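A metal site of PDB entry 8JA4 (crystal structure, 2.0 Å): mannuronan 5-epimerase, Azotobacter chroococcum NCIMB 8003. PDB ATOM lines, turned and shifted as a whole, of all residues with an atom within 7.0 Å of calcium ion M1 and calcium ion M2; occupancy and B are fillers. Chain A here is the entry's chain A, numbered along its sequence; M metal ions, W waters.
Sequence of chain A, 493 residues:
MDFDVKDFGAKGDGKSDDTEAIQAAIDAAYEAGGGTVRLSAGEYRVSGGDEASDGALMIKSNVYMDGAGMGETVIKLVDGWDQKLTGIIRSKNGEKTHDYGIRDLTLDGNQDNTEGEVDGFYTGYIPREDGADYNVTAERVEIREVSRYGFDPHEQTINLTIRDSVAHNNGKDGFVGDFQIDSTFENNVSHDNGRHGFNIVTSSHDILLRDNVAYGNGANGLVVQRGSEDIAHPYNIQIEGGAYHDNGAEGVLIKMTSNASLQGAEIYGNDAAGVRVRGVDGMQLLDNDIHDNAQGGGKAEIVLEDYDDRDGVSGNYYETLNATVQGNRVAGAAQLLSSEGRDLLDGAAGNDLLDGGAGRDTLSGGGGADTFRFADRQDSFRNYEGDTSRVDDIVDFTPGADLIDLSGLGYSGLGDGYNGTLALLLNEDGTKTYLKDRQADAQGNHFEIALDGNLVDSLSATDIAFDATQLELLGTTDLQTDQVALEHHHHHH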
ATOM      1  N   LEU A 321      -4.281 -24.498  -1.452  1.00  0.00           N
ATOM      2  CA  LEU A 321      -3.770 -24.709  -0.115  1.00  0.00           C
ATOM      3  C   LEU A 321      -2.339 -25.201  -0.173  1.00  0.00           C
ATOM      4  O   LEU A 321      -1.920 -25.806  -1.175  1.00  0.00           O
ATOM      5  CB  LEU A 321      -4.563 -25.806   0.619  1.00  0.00           C
ATOM      6  CG  LEU A 321      -6.059 -25.599   0.714  1.00  0.00           C
ATOM      7  CD1 LEU A 321      -6.733 -26.937   0.948  1.00  0.00           C
ATOM      8  CD2 LEU A 321      -6.270 -24.667   1.921  1.00  0.00           C
ATOM      9  N   ASN A 322      -1.653 -25.185   0.967  1.00  0.00           N
ATOM     10  CA  ASN A 322      -0.311 -25.813   1.093  1.00  0.00           C
ATOM     11  C   ASN A 322       0.579 -25.419  -0.084  1.00  0.00           C
ATOM     12  O   ASN A 322       1.062 -26.312  -0.792  1.00  0.00           O
ATOM     13  CB  ASN A 322      -0.433 -27.320   1.285  1.00  0.00           C
ATOM     14  CG  ASN A 322      -1.326 -27.720   2.447  1.00  0.00           C
ATOM     15  OD1 ASN A 322      -1.064 -27.353   3.591  1.00  0.00           O
ATOM     16  ND2 ASN A 322      -2.374 -28.477   2.167  1.00  0.00           N
ATOM     17  N   SER A 338      -3.444 -17.947  -0.745  1.00  0.00           N
ATOM     18  CA  SER A 338      -3.642 -19.310  -0.276  1.00  0.00           C
ATOM     19  C   SER A 338      -4.545 -19.269   0.962  1.00  0.00           C
ATOM     20  O   SER A 338      -5.033 -18.218   1.399  1.00  0.00           O
ATOM     21  CB  SER A 338      -2.259 -19.945  -0.044  1.00  0.00           C
ATOM     22  OG  SER A 338      -2.440 -21.332   0.167  1.00  0.00           O
ATOM     23  N   SER A 339      -4.731 -20.405   1.629  1.00  0.00           N
ATOM     24  CA  SER A 339      -5.776 -20.546   2.659  1.00  0.00           C
ATOM     25  C   SER A 339      -5.195 -21.336   3.833  1.00  0.00           C
ATOM     26  O   SER A 339      -4.000 -21.276   4.110  1.00  0.00           O
ATOM     27  CB  SER A 339      -7.038 -21.170   2.052  1.00  0.00           C
ATOM     28  OG  SER A 339      -8.143 -21.001   2.930  1.00  0.00           O
ATOM     29  N   GLU A 340      -6.107 -21.972   4.585  1.00  0.00           N
ATOM     30  CA  GLU A 340      -5.738 -22.715   5.810  1.00  0.00           C
ATOM     31  C   GLU A 340      -4.407 -23.557   5.726  1.00  0.00           C
ATOM     32  O   GLU A 340      -4.017 -24.310   4.760  1.00  0.00           O
ATOM     33  CB  GLU A 340      -6.884 -23.575   6.335  1.00  0.00           C
ATOM     34  CG  GLU A 340      -7.696 -24.264   5.254  1.00  0.00           C
ATOM     35  CD  GLU A 340      -9.030 -23.594   5.014  1.00  0.00           C
ATOM     36  OE1 GLU A 340     -10.035 -24.319   4.899  1.00  0.00           O
ATOM     37  OE2 GLU A 340      -9.064 -22.348   4.967  1.00  0.00           O
ATOM     38  N   GLY A 341      -3.667 -23.460   6.824  1.00  0.00           N
ATOM     39  CA  GLY A 341      -2.382 -24.123   6.814  1.00  0.00           C
ATOM     40  C   GLY A 341      -1.264 -23.150   6.472  1.00  0.00           C
ATOM     41  O   GLY A 341      -1.486 -21.990   6.138  1.00  0.00           O
ATOM     42  N   ARG A 342      -0.034 -23.662   6.581  1.00  0.00           N
ATOM     43  CA  ARG A 342       1.180 -22.845   6.472  1.00  0.00           C
ATOM     44  C   ARG A 342       1.580 -22.723   5.006  1.00  0.00           C
ATOM     45  O   ARG A 342       1.838 -23.744   4.357  1.00  0.00           O
ATOM     46  CB  ARG A 342       2.298 -23.511   7.288  1.00  0.00           C
ATOM     47  CG  ARG A 342       3.687 -22.927   7.004  1.00  0.00           C
ATOM     48  CD  ARG A 342       4.511 -22.911   8.286  1.00  0.00           C
ATOM     49  NE  ARG A 342       5.851 -22.380   8.049  1.00  0.00           N
ATOM     50  CZ  ARG A 342       6.143 -21.077   8.006  1.00  0.00           C
ATOM     51  NH1 ARG A 342       5.177 -20.149   8.076  1.00  0.00           N
ATOM     52  NH2 ARG A 342       7.424 -20.696   7.899  1.00  0.00           N
ATOM     53  N   ASP A 343       1.646 -21.493   4.491  1.00  0.00           N
ATOM     54  CA  ASP A 343       2.107 -21.207   3.130  1.00  0.00           C
ATOM     55  C   ASP A 343       3.416 -20.431   3.147  1.00  0.00           C
ATOM     56  O   ASP A 343       3.657 -19.605   4.032  1.00  0.00           O
ATOM     57  CB  ASP A 343       1.030 -20.409   2.397  1.00  0.00           C
ATOM     58  CG  ASP A 343      -0.263 -21.224   2.256  1.00  0.00           C
ATOM     59  OD1 ASP A 343      -0.376 -22.024   1.286  1.00  0.00           O
ATOM     60  OD2 ASP A 343      -1.132 -21.112   3.160  1.00  0.00           O
ATOM     61  N   LEU A 345       5.269 -17.936   0.672  1.00  0.00           N
ATOM     62  CA  LEU A 345       4.890 -17.213  -0.549  1.00  0.00           C
ATOM     63  C   LEU A 345       5.904 -16.109  -0.833  1.00  0.00           C
ATOM     64  O   LEU A 345       5.943 -15.089  -0.127  1.00  0.00           O
ATOM     65  CB  LEU A 345       3.467 -16.655  -0.413  1.00  0.00           C
ATOM     66  CG  LEU A 345       2.364 -17.691  -0.127  1.00  0.00           C
ATOM     67  CD1 LEU A 345       0.975 -17.025   0.059  1.00  0.00           C
ATOM     68  CD2 LEU A 345       2.302 -18.691  -1.277  1.00  0.00           C
ATOM     69  N   ASP A 355      -1.202 -12.958   0.053  1.00  0.00           N
ATOM     70  CA  ASP A 355      -2.127 -13.229   1.162  1.00  0.00           C
ATOM     71  C   ASP A 355      -2.085 -14.729   1.439  1.00  0.00           C
ATOM     72  O   ASP A 355      -2.683 -15.497   0.676  1.00  0.00           O
ATOM     73  CB  ASP A 355      -3.560 -12.780   0.822  1.00  0.00           C
ATOM     74  CG  ASP A 355      -4.558 -12.988   1.989  1.00  0.00           C
ATOM     75  OD1 ASP A 355      -4.258 -13.690   3.015  1.00  0.00           O
ATOM     76  OD2 ASP A 355      -5.641 -12.389   1.938  1.00  0.00           O
ATOM     77  N   GLY A 356      -1.476 -15.141   2.559  1.00  0.00           N
ATOM     78  CA  GLY A 356      -1.493 -16.560   2.947  1.00  0.00           C
ATOM     79  C   GLY A 356      -2.776 -17.059   3.593  1.00  0.00           C
ATOM     80  O   GLY A 356      -2.878 -18.267   3.926  1.00  0.00           O
ATOM     81  N   GLY A 357      -3.738 -16.172   3.857  1.00  0.00           N
ATOM     82  CA  GLY A 357      -4.994 -16.740   4.416  1.00  0.00           C
ATOM     83  C   GLY A 357      -4.792 -17.294   5.820  1.00  0.00           C
ATOM     84  O   GLY A 357      -3.831 -16.969   6.519  1.00  0.00           O
ATOM     85  N   ALA A 358      -5.734 -18.142   6.263  1.00  0.00           N
ATOM     86  CA  ALA A 358      -5.641 -18.727   7.606  1.00  0.00           C
ATOM     87  C   ALA A 358      -4.310 -19.455   7.827  1.00  0.00           C
ATOM     88  O   ALA A 358      -3.598 -19.808   6.863  1.00  0.00           O
ATOM     89  CB  ALA A 358      -6.821 -19.685   7.823  1.00  0.00           C
ATOM     90  N   GLY A 359      -3.923 -19.654   9.105  1.00  0.00           N
ATOM     91  CA  GLY A 359      -2.689 -20.354   9.428  1.00  0.00           C
ATOM     92  C   GLY A 359      -1.461 -19.460   9.334  1.00  0.00           C
ATOM     93  O   GLY A 359      -1.530 -18.283   8.992  1.00  0.00           O
ATOM     94  N   ARG A 360      -0.306 -20.058   9.630  1.00  0.00           N
ATOM     95  CA  ARG A 360       0.913 -19.288   9.850  1.00  0.00           C
ATOM     96  C   ARG A 360       1.758 -19.283   8.587  1.00  0.00           C
ATOM     97  O   ARG A 360       2.387 -20.294   8.241  1.00  0.00           O
ATOM     98  CB  ARG A 360       1.700 -19.828  11.047  1.00  0.00           C
ATOM     99  CG  ARG A 360       2.965 -18.977  11.341  1.00  0.00           C
ATOM    100  CD  ARG A 360       3.739 -19.556  12.538  1.00  0.00           C
ATOM    101  NE  ARG A 360       4.551 -20.702  12.138  1.00  0.00           N
ATOM    102  CZ  ARG A 360       5.785 -20.644  11.620  1.00  0.00           C
ATOM    103  NH1 ARG A 360       6.395 -19.481  11.388  1.00  0.00           N
ATOM    104  NH2 ARG A 360       6.402 -21.782  11.299  1.00  0.00           N
ATOM    105  N   ASP A 361       1.824 -18.139   7.932  1.00  0.00           N
ATOM    106  CA  ASP A 361       2.489 -17.995   6.645  1.00  0.00           C
ATOM    107  C   ASP A 361       3.744 -17.133   6.739  1.00  0.00           C
ATOM    108  O   ASP A 361       3.858 -16.234   7.577  1.00  0.00           O
ATOM    109  CB  ASP A 361       1.513 -17.335   5.686  1.00  0.00           C
ATOM    110  CG  ASP A 361       0.166 -17.975   5.748  1.00  0.00           C
ATOM    111  OD1 ASP A 361       0.132 -19.187   5.530  1.00  0.00           O
ATOM    112  OD2 ASP A 361      -0.842 -17.284   6.002  1.00  0.00           O
ATOM    113  N   THR A 362       4.670 -17.375   5.813  1.00  0.00           N
ATOM    114  CA  THR A 362       5.880 -16.572   5.672  1.00  0.00           C
ATOM    115  C   THR A 362       5.839 -16.003   4.266  1.00  0.00           C
ATOM    116  O   THR A 362       5.811 -16.766   3.295  1.00  0.00           O
ATOM    117  CB  THR A 362       7.126 -17.429   5.890  1.00  0.00           C
ATOM    118  OG1 THR A 362       7.063 -17.994   7.213  1.00  0.00           O
ATOM    119  CG2 THR A 362       8.373 -16.588   5.785  1.00  0.00           C
ATOM    120  N   LEU A 363       5.832 -14.659   4.166  1.00  0.00           N
ATOM    121  CA  LEU A 363       5.636 -13.913   2.938  1.00  0.00           C
ATOM    122  C   LEU A 363       6.875 -13.057   2.663  1.00  0.00           C
ATOM    123  O   LEU A 363       7.503 -12.524   3.593  1.00  0.00           O
ATOM    124  CB  LEU A 363       4.382 -12.987   3.001  1.00  0.00           C
ATOM    125  CG  LEU A 363       3.172 -13.632   3.694  1.00  0.00           C
ATOM    126  CD1 LEU A 363       2.096 -12.625   4.131  1.00  0.00           C
ATOM    127  CD2 LEU A 363       2.542 -14.651   2.715  1.00  0.00           C
ATOM    128  N   PHE A 374      -4.069  -8.875   4.632  1.00  0.00           N
ATOM    129  CA  PHE A 374      -4.548  -9.679   5.750  1.00  0.00           C
ATOM    130  C   PHE A 374      -6.058  -9.485   5.764  1.00  0.00           C
ATOM    131  O   PHE A 374      -6.569  -8.412   6.112  1.00  0.00           O
ATOM    132  CB  PHE A 374      -3.853  -9.263   7.052  1.00  0.00           C
ATOM    133  CG  PHE A 374      -2.395  -9.563   7.040  1.00  0.00           C
ATOM    134  CD1 PHE A 374      -1.924 -10.749   7.550  1.00  0.00           C
ATOM    135  CD2 PHE A 374      -1.510  -8.691   6.423  1.00  0.00           C
ATOM    136  CE1 PHE A 374      -0.553 -11.030   7.471  1.00  0.00           C
ATOM    137  CE2 PHE A 374      -0.195  -8.961   6.334  1.00  0.00           C
ATOM    138  CZ  PHE A 374       0.299 -10.142   6.852  1.00  0.00           C
ATOM    139  N   GLN A 378      -8.468 -13.352  12.153  1.00  0.00           N
ATOM    140  CA  GLN A 378      -8.075 -14.685  12.584  1.00  0.00           C
ATOM    141  C   GLN A 378      -7.024 -15.309  11.649  1.00  0.00           C
ATOM    142  O   GLN A 378      -6.659 -16.452  11.832  1.00  0.00           O
ATOM    143  CB  GLN A 378      -9.291 -15.609  12.715  1.00  0.00           C
ATOM    144  CG  GLN A 378     -10.230 -15.265  13.864  1.00  0.00           C
ATOM    145  CD  GLN A 378      -9.605 -15.457  15.267  1.00  0.00           C
ATOM    146  OE1 GLN A 378      -9.579 -14.526  16.121  1.00  0.00           O
ATOM    147  NE2 GLN A 378      -9.142 -16.697  15.535  1.00  0.00           N
ATOM    148  N   ASP A 379      -6.503 -14.565  10.691  1.00  0.00           N
ATOM    149  CA  ASP A 379      -5.510 -15.110   9.774  1.00  0.00           C
ATOM    150  C   ASP A 379      -4.055 -14.920  10.216  1.00  0.00           C
ATOM    151  O   ASP A 379      -3.146 -15.449   9.550  1.00  0.00           O
ATOM    152  CB  ASP A 379      -5.674 -14.464   8.394  1.00  0.00           C
ATOM    153  CG  ASP A 379      -6.916 -14.992   7.603  1.00  0.00           C
ATOM    154  OD1 ASP A 379      -7.589 -15.998   8.042  1.00  0.00           O
ATOM    155  OD2 ASP A 379      -7.177 -14.390   6.528  1.00  0.00           O
ATOM    156  N   SER A 380      -3.818 -14.139  11.272  1.00  0.00           N
ATOM    157  CA  SER A 380      -2.477 -13.926  11.801  1.00  0.00           C
ATOM    158  C   SER A 380      -2.732 -13.487  13.233  1.00  0.00           C
ATOM    159  O   SER A 380      -3.231 -12.373  13.417  1.00  0.00           O
ATOM    160  CB  SER A 380      -1.731 -12.866  10.981  1.00  0.00           C
ATOM    161  OG  SER A 380      -0.363 -12.759  11.394  1.00  0.00           O
ATOM    162  N   PHE A 381      -2.461 -14.348  14.198  1.00  0.00           N
ATOM    163  CA  PHE A 381      -2.840 -13.991  15.581  1.00  0.00           C
ATOM    164  C   PHE A 381      -2.015 -14.735  16.627  1.00  0.00           C
ATOM    165  O   PHE A 381      -1.370 -15.744  16.310  1.00  0.00           O
ATOM    166  CB  PHE A 381      -4.312 -14.313  15.813  1.00  0.00           C
ATOM    167  CG  PHE A 381      -4.632 -15.780  15.823  1.00  0.00           C
ATOM    168  CD1 PHE A 381      -4.880 -16.451  14.638  1.00  0.00           C
ATOM    169  CD2 PHE A 381      -4.691 -16.494  17.007  1.00  0.00           C
ATOM    170  CE1 PHE A 381      -5.183 -17.807  14.642  1.00  0.00           C
ATOM    171  CE2 PHE A 381      -4.992 -17.839  17.014  1.00  0.00           C
ATOM    172  CZ  PHE A 381      -5.237 -18.491  15.832  1.00  0.00           C
ATOM    173  N   ARG A 390       0.805 -19.114  14.748  1.00  0.00           N
ATOM    174  CA  ARG A 390      -0.343 -18.531  14.009  1.00  0.00           C
ATOM    175  C   ARG A 390      -0.040 -17.064  13.709  1.00  0.00           C
ATOM    176  O   ARG A 390      -0.902 -16.404  13.116  1.00  0.00           O
ATOM    177  CB  ARG A 390      -1.644 -18.743  14.786  1.00  0.00           C
ATOM    178  CG  ARG A 390      -1.915 -20.205  15.143  1.00  0.00           C
ATOM    179  CD  ARG A 390      -1.528 -21.142  14.017  1.00  0.00           C
ATOM    180  NE  ARG A 390      -1.018 -22.408  14.531  1.00  0.00           N
ATOM    181  CZ  ARG A 390      -1.718 -23.248  15.294  1.00  0.00           C
ATOM    182  NH1 ARG A 390      -2.955 -22.948  15.633  1.00  0.00           N
ATOM    183  NH2 ARG A 390      -1.178 -24.375  15.706  1.00  0.00           N
ATOM    184  N   VAL A 391       1.147 -16.585  14.066  1.00  0.00           N
ATOM    185  CA  VAL A 391       1.542 -15.193  13.698  1.00  0.00           C
ATOM    186  C   VAL A 391       2.343 -15.223  12.393  1.00  0.00           C
ATOM    187  O   VAL A 391       3.446 -15.775  12.396  1.00  0.00           O
ATOM    188  CB  VAL A 391       2.319 -14.464  14.817  1.00  0.00           C
ATOM    189  CG1 VAL A 391       2.821 -13.121  14.343  1.00  0.00           C
ATOM    190  CG2 VAL A 391       1.472 -14.301  16.070  1.00  0.00           C
ATOM    191  N   ASP A 392       1.785 -14.648  11.341  1.00  0.00           N
ATOM    192  CA  ASP A 392       2.477 -14.521  10.064  1.00  0.00           C
ATOM    193  C   ASP A 392       3.748 -13.657  10.187  1.00  0.00           C
ATOM    194  O   ASP A 392       3.786 -12.667  10.945  1.00  0.00           O
ATOM    195  CB  ASP A 392       1.582 -13.858   9.018  1.00  0.00           C
ATOM    196  CG  ASP A 392       0.473 -14.773   8.498  1.00  0.00           C
ATOM    197  OD1 ASP A 392       0.188 -15.859   9.048  1.00  0.00           O
ATOM    198  OD2 ASP A 392      -0.102 -14.392   7.450  1.00  0.00           O
HETATM  199 CA    CA M   1      -2.109 -20.101   5.039  1.00  0.00          CA
HETATM  200 CA    CA M   2      -1.918 -16.181   7.765  1.00  0.00          CA
HETATM  201  O   HOH W   1      -2.693 -14.234   6.610  1.00  0.00           O
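OD1 of Asp 379 lies within hydrogen-bond range of N of Ala 358 (3.3 Å). OG of Ser 338 lies within hydrogen-bond range of OD1 of Asp 343 (2.4 Å). N of Asn 322 sits at hydrogen-bond distance from OD1 of Asp 343, at 3.4 Å. O of Asp 343 sits at hydrogen-bond distance from N of Thr 362 (3.0 Å). OE2 of Glu 340 lies within hydrogen-bond range of OG of Ser 339 (2.6 Å). N of Gly 357 sits close to O of Ser 338, at 3.5 Å. The backbone NH (N) of Gly 357 sits at hydrogen-bond distance from the side-chain carboxylate (OD1) of Asp 355. N of Asp 392 sits at hydrogen-bond distance from OG of Ser 380 (2.9 Å).
Within 4 Å of calcium ion M1: Ser 339, Gly 341, Asp 343, Gly 356, Gly 357, Ala 358 and Asp 361.
Five residues have an atom within 4 Å of calcium ion M2: Gly 357, Gly 359, Asp 361, Asp 379 and Asp 392. The nearest printed residue that does not touch calcium ion M2 is Ala 358 (4.1 Å).
Calcium ion M1 is bound by the backbone carbonyl oxygen of Gly 341 (2.3 Å), the backbone carbonyl oxygen of Gly 356 (2.3 Å), the side-chain carboxylate of Asp 343 (2.3 Å), the backbone carbonyl oxygen of Ala 358 (2.4 Å), the backbone carbonyl oxygen of Ser 339 (2.4 Å) and the side-chain carboxylate of Asp 361 (2.5 Å). Calcium ion M1 has six donor atoms within binding distance.
Calcium ion M2 is bound by O of Asp 379 (2.3 Å). OD2 of Asp 361 is bound to calcium ion M2 (2.3 Å). Water W1 is bound to calcium ion M2. O of Gly 357 is bound to calcium ion M2, at 2.4 Å. O of Gly 359 is bound to calcium ion M2 (2.5 Å). Calcium ion M2 is bound by OD1 of Asp 392. Calcium ion M2 is bound by the side-chain carboxylate (OD2) of Asp 392 (2.6 Å).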
